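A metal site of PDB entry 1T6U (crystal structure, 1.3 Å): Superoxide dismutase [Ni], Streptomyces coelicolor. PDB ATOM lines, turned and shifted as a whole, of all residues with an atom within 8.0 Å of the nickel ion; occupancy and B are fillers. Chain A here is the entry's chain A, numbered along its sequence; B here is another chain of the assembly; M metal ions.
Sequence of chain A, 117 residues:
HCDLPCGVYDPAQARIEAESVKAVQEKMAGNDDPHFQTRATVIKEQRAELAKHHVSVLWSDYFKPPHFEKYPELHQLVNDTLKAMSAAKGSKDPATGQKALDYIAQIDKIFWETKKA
N of His 1 lies close to O of Val 8 (3.0 Å).
The side-chain hydroxyl (OG) of Ser 20 of chain B sits close to a ring nitrogen (NE2) of His 1, at 3.3 Å.
NE of Arg 47 of chain B sits at hydrogen-bond distance from NE2 of His 1 (3.5 Å).
A ring nitrogen (NE2) of His 1 is in hydrogen-bond range of the side-chain carboxylate (OE2) of Glu 17 of chain B (2.8 Å).
N of Val 8 sits close to SG of Cys 6 (3.3 Å).
Residues that only touch the nickel ion: Asp 3.
Within 4 Å of the nickel ion: His 1, Cys 2, Asp 3 and Cys 6.
The nearest printed residue that does not touch the nickel ion is Val 8 (4.2 Å).
The nickel ion is bound by the backbone nitrogen (N) of His 1, the backbone nitrogen (N) of Cys 2, the side-chain sulfur (SG) of Cys 2, the side-chain sulfur (SG) of Cys 6 and a ring nitrogen (ND1) of His 1.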
ATOM      1  N   HIS A   1       6.452  17.942 -10.963  1.00  0.00           N
ATOM      2  CA  HIS A   1       5.537  16.781 -10.985  1.00  0.00           C
ATOM      3  C   HIS A   1       6.361  15.536 -11.274  1.00  0.00           C
ATOM      4  O   HIS A   1       5.939  14.390 -11.180  1.00  0.00           O
ATOM      5  CB  HIS A   1       4.466  16.942 -12.058  1.00  0.00           C
ATOM      6  CG  HIS A   1       5.001  17.115 -13.461  1.00  0.00           C
ATOM      7  ND1 HIS A   1       6.352  17.365 -13.659  1.00  0.00           N
ATOM      8  CD2 HIS A   1       4.443  17.088 -14.693  1.00  0.00           C
ATOM      9  CE1 HIS A   1       6.567  17.474 -14.965  1.00  0.00           C
ATOM     10  NE2 HIS A   1       5.417  17.321 -15.617  1.00  0.00           N
ATOM     11  N   CYS A   2       7.590  15.840 -11.683  1.00  0.00           N
ATOM     12  CA  CYS A   2       8.531  14.820 -12.156  1.00  0.00           C
ATOM     13  C   CYS A   2       9.582  14.423 -11.127  1.00  0.00           C
ATOM     14  O   CYS A   2      10.436  13.615 -11.465  1.00  0.00           O
ATOM     15  CB  CYS A   2       9.270  15.397 -13.365  1.00  0.00           C
ATOM     16  SG  CYS A   2       9.802  17.073 -13.009  1.00  0.00           S
ATOM     17  N   ASP A   3       9.556  15.041  -9.942  1.00  0.00           N
ATOM     18  CA  ASP A   3      10.400  14.716  -8.787  1.00  0.00           C
ATOM     19  C   ASP A   3      11.838  15.221  -8.944  1.00  0.00           C
ATOM     20  O   ASP A   3      12.737  14.759  -8.231  1.00  0.00           O
ATOM     21  CB  ASP A   3      10.364  13.216  -8.524  1.00  0.00           C
ATOM     22  CG  ASP A   3      10.303  12.774  -7.074  1.00  0.00           C
ATOM     23  OD1 ASP A   3      10.358  13.593  -6.153  1.00  0.00           O
ATOM     24  OD2 ASP A   3      10.184  11.513  -6.925  1.00  0.00           O
ATOM     25  N   LEU A   4      12.056  16.198  -9.822  1.00  0.00           N
ATOM     26  CA  LEU A   4      13.417  16.726  -9.929  1.00  0.00           C
ATOM     27  C   LEU A   4      13.885  17.411  -8.668  1.00  0.00           C
ATOM     28  O   LEU A   4      15.022  17.107  -8.204  1.00  0.00           O
ATOM     29  CB  LEU A   4      13.567  17.671 -11.149  1.00  0.00           C
ATOM     30  CG  LEU A   4      14.953  18.324 -11.193  1.00  0.00           C
ATOM     31  CD1 LEU A   4      16.042  17.291 -11.413  1.00  0.00           C
ATOM     32  CD2 LEU A   4      15.070  19.410 -12.277  1.00  0.00           C
ATOM     33  N   PRO A   5      13.140  18.327  -8.051  1.00  0.00           N
ATOM     34  CA  PRO A   5      11.832  18.846  -8.405  1.00  0.00           C
ATOM     35  C   PRO A   5      11.830  19.892  -9.515  1.00  0.00           C
ATOM     36  O   PRO A   5      12.767  20.694  -9.634  1.00  0.00           O
ATOM     37  CB  PRO A   5      11.355  19.485  -7.082  1.00  0.00           C
ATOM     38  CG  PRO A   5      12.632  19.962  -6.457  1.00  0.00           C
ATOM     39  CD  PRO A   5      13.691  18.938  -6.805  1.00  0.00           C
ATOM     40  N   CYS A   6      10.744  19.899 -10.317  1.00  0.00           N
ATOM     41  CA  CYS A   6      10.594  20.926 -11.337  1.00  0.00           C
ATOM     42  C   CYS A   6       9.747  22.097 -10.887  1.00  0.00           C
ATOM     43  O   CYS A   6       9.811  23.138 -11.532  1.00  0.00           O
ATOM     44  CB  CYS A   6       9.990  20.340 -12.625  1.00  0.00           C
ATOM     45  SG  CYS A   6       8.267  19.844 -12.447  1.00  0.00           S
ATOM     46  N   GLY A   7       8.997  21.954  -9.819  1.00  0.00           N
ATOM     47  CA  GLY A   7       8.115  22.990  -9.311  1.00  0.00           C
ATOM     48  C   GLY A   7       6.819  23.180 -10.072  1.00  0.00           C
ATOM     49  O   GLY A   7       6.070  24.085  -9.698  1.00  0.00           O
ATOM     50  N   VAL A   8       6.536  22.353 -11.062  1.00  0.00           N
ATOM     51  CA  VAL A   8       5.318  22.437 -11.862  1.00  0.00           C
ATOM     52  C   VAL A   8       4.305  21.375 -11.413  1.00  0.00           C
ATOM     53  O   VAL A   8       4.582  20.191 -11.480  1.00  0.00           O
ATOM     54  CB  VAL A   8       5.604  22.268 -13.361  1.00  0.00           C
ATOM     55  CG1 VAL A   8       4.335  22.330 -14.208  1.00  0.00           C
ATOM     56  CG2 VAL A   8       6.538  23.366 -13.829  1.00  0.00           C
ATOM     57  N   TYR A   9       3.169  21.846 -10.949  1.00  0.00           N
ATOM     58  CA  TYR A   9       2.063  20.966 -10.584  1.00  0.00           C
ATOM     59  C   TYR A   9       0.731  21.559 -10.951  1.00  0.00           C
ATOM     60  O   TYR A   9       0.544  22.771 -10.905  1.00  0.00           O
ATOM     61  CB  TYR A   9       1.970  20.703  -9.066  1.00  0.00           C
ATOM     62  CG  TYR A   9       3.202  20.105  -8.448  1.00  0.00           C
ATOM     63  CD1 TYR A   9       4.240  20.909  -8.034  1.00  0.00           C
ATOM     64  CD2 TYR A   9       3.319  18.738  -8.333  1.00  0.00           C
ATOM     65  CE1 TYR A   9       5.355  20.324  -7.482  1.00  0.00           C
ATOM     66  CE2 TYR A   9       4.433  18.153  -7.781  1.00  0.00           C
ATOM     67  CZ  TYR A   9       5.444  18.970  -7.362  1.00  0.00           C
ATOM     68  OH  TYR A   9       6.577  18.416  -6.804  1.00  0.00           O
ATOM     69  N   GLN A  13      -4.012  17.525 -14.288  1.00  0.00           N
ATOM     70  CA  GLN A  13      -3.516  16.282 -14.868  1.00  0.00           C
ATOM     71  C   GLN A  13      -4.387  15.116 -14.404  1.00  0.00           C
ATOM     72  O   GLN A  13      -4.819  14.324 -15.242  1.00  0.00           O
ATOM     73  CB  GLN A  13      -2.033  16.022 -14.546  1.00  0.00           C
ATOM     74  CG  GLN A  13      -1.085  17.127 -14.990  1.00  0.00           C
ATOM     75  CD  GLN A  13       0.359  16.657 -14.922  1.00  0.00           C
ATOM     76  OE1 GLN A  13       1.002  16.647 -13.843  1.00  0.00           O
ATOM     77  NE2 GLN A  13       0.908  16.292 -16.072  1.00  0.00           N
ATOM     78  N   VAL A  57       1.229  11.734  -6.663  1.00  0.00           N
ATOM     79  CA  VAL A  57       2.317  12.687  -6.780  1.00  0.00           C
ATOM     80  C   VAL A  57       1.981  14.018  -6.109  1.00  0.00           C
ATOM     81  O   VAL A  57       2.811  14.623  -5.427  1.00  0.00           O
ATOM     82  CB  VAL A  57       2.647  12.862  -8.286  1.00  0.00           C
ATOM     83  CG1 VAL A  57       3.448  14.125  -8.527  1.00  0.00           C
ATOM     84  CG2 VAL A  57       3.395  11.635  -8.831  1.00  0.00           C
ATOM     85  N   ASP A  61       4.607  14.720  -3.303  1.00  0.00           N
ATOM     86  CA  ASP A  61       5.660  15.607  -3.790  1.00  0.00           C
ATOM     87  C   ASP A  61       5.303  17.080  -3.681  1.00  0.00           C
ATOM     88  O   ASP A  61       6.188  17.854  -3.351  1.00  0.00           O
ATOM     89  CB  ASP A  61       5.958  15.238  -5.253  1.00  0.00           C
ATOM     90  CG  ASP A  61       6.562  13.869  -5.483  1.00  0.00           C
ATOM     91  OD1 ASP A  61       6.643  13.033  -4.581  1.00  0.00           O
ATOM     92  OD2 ASP A  61       6.955  13.610  -6.650  1.00  0.00           O
ATOM     93  N   ILE B  16       1.399  21.572 -19.956  1.00  0.00           N
ATOM     94  CA  ILE B  16       2.048  21.408 -18.644  1.00  0.00           C
ATOM     95  C   ILE B  16       3.368  20.643 -18.762  1.00  0.00           C
ATOM     96  O   ILE B  16       4.316  20.946 -18.024  1.00  0.00           O
ATOM     97  CB  ILE B  16       1.102  20.701 -17.648  1.00  0.00           C
ATOM     98  CG1 ILE B  16       1.564  20.747 -16.181  1.00  0.00           C
ATOM     99  CG2 ILE B  16       0.867  19.241 -18.014  1.00  0.00           C
ATOM    100  CD1 ILE B  16       0.502  20.870 -15.117  1.00  0.00           C
ATOM    101  N   GLU B  17       3.456  19.629 -19.643  1.00  0.00           N
ATOM    102  CA  GLU B  17       4.739  18.947 -19.820  1.00  0.00           C
ATOM    103  C   GLU B  17       5.768  19.900 -20.412  1.00  0.00           C
ATOM    104  O   GLU B  17       6.919  19.875 -19.978  1.00  0.00           O
ATOM    105  CB  GLU B  17       4.546  17.687 -20.649  1.00  0.00           C
ATOM    106  CG  GLU B  17       3.664  16.634 -19.978  1.00  0.00           C
ATOM    107  CD  GLU B  17       4.151  16.157 -18.628  1.00  0.00           C
ATOM    108  OE1 GLU B  17       3.347  15.493 -17.894  1.00  0.00           O
ATOM    109  OE2 GLU B  17       5.320  16.434 -18.260  1.00  0.00           O
ATOM    110  N   SER B  20       7.067  22.045 -17.729  1.00  0.00           N
ATOM    111  CA  SER B  20       8.051  21.360 -16.874  1.00  0.00           C
ATOM    112  C   SER B  20       9.369  21.291 -17.608  1.00  0.00           C
ATOM    113  O   SER B  20      10.437  21.473 -16.964  1.00  0.00           O
ATOM    114  CB  SER B  20       7.516  20.009 -16.383  1.00  0.00           C
ATOM    115  OG  SER B  20       7.614  19.043 -17.385  1.00  0.00           O
ATOM    116  N   VAL B  21       9.421  21.070 -18.922  1.00  0.00           N
ATOM    117  CA  VAL B  21      10.683  21.109 -19.659  1.00  0.00           C
ATOM    118  C   VAL B  21      11.392  22.448 -19.504  1.00  0.00           C
ATOM    119  O   VAL B  21      12.614  22.495 -19.219  1.00  0.00           O
ATOM    120  CB  VAL B  21      10.424  20.785 -21.136  1.00  0.00           C
ATOM    121  CG1 VAL B  21      11.644  21.101 -21.996  1.00  0.00           C
ATOM    122  CG2 VAL B  21       9.961  19.322 -21.301  1.00  0.00           C
ATOM    123  N   ALA B  23      10.965  24.675 -17.091  1.00  0.00           N
ATOM    124  CA  ALA B  23      11.344  24.825 -15.702  1.00  0.00           C
ATOM    125  C   ALA B  23      12.616  24.055 -15.388  1.00  0.00           C
ATOM    126  O   ALA B  23      13.507  24.548 -14.681  1.00  0.00           O
ATOM    127  CB  ALA B  23      10.241  24.351 -14.780  1.00  0.00           C
ATOM    128  N   VAL B  24      12.715  22.846 -15.927  1.00  0.00           N
ATOM    129  CA  VAL B  24      13.938  22.055 -15.746  1.00  0.00           C
ATOM    130  C   VAL B  24      15.133  22.784 -16.315  1.00  0.00           C
ATOM    131  O   VAL B  24      16.167  22.876 -15.660  1.00  0.00           O
ATOM    132  CB  VAL B  24      13.766  20.647 -16.320  1.00  0.00           C
ATOM    133  CG1 VAL B  24      15.084  19.898 -16.288  1.00  0.00           C
ATOM    134  CG2 VAL B  24      12.720  19.912 -15.510  1.00  0.00           C
ATOM    135  N   ILE B  43      15.064  13.710 -16.684  1.00  0.00           N
ATOM    136  CA  ILE B  43      13.688  14.104 -16.519  1.00  0.00           C
ATOM    137  C   ILE B  43      13.185  14.997 -17.635  1.00  0.00           C
ATOM    138  O   ILE B  43      12.058  14.833 -18.119  1.00  0.00           O
ATOM    139  CB  ILE B  43      13.535  14.765 -15.129  1.00  0.00           C
ATOM    140  CG1 ILE B  43      13.595  13.673 -14.053  1.00  0.00           C
ATOM    141  CG2 ILE B  43      12.285  15.603 -15.074  1.00  0.00           C
ATOM    142  CD1 ILE B  43      13.873  14.254 -12.663  1.00  0.00           C
ATOM    143  N   ARG B  47       9.856  14.268 -19.944  1.00  0.00           N
ATOM    144  CA  ARG B  47       8.681  15.156 -20.026  1.00  0.00           C
ATOM    145  C   ARG B  47       8.531  15.683 -21.436  1.00  0.00           C
ATOM    146  O   ARG B  47       7.404  15.853 -21.940  1.00  0.00           O
ATOM    147  CB  ARG B  47       8.754  16.311 -19.026  1.00  0.00           C
ATOM    148  CG  ARG B  47       9.110  15.927 -17.594  1.00  0.00           C
ATOM    149  CD  ARG B  47       8.484  14.639 -17.105  1.00  0.00           C
ATOM    150  NE  ARG B  47       7.038  14.593 -17.021  1.00  0.00           N
ATOM    151  CZ  ARG B  47       6.341  13.737 -16.277  1.00  0.00           C
ATOM    152  NH1 ARG B  47       6.990  12.841 -15.550  1.00  0.00           N
ATOM    153  NH2 ARG B  47       5.006  13.757 -16.253  1.00  0.00           N
HETATM  154 NI    NI M   1       7.974  17.697 -12.043  1.00  0.00          NI
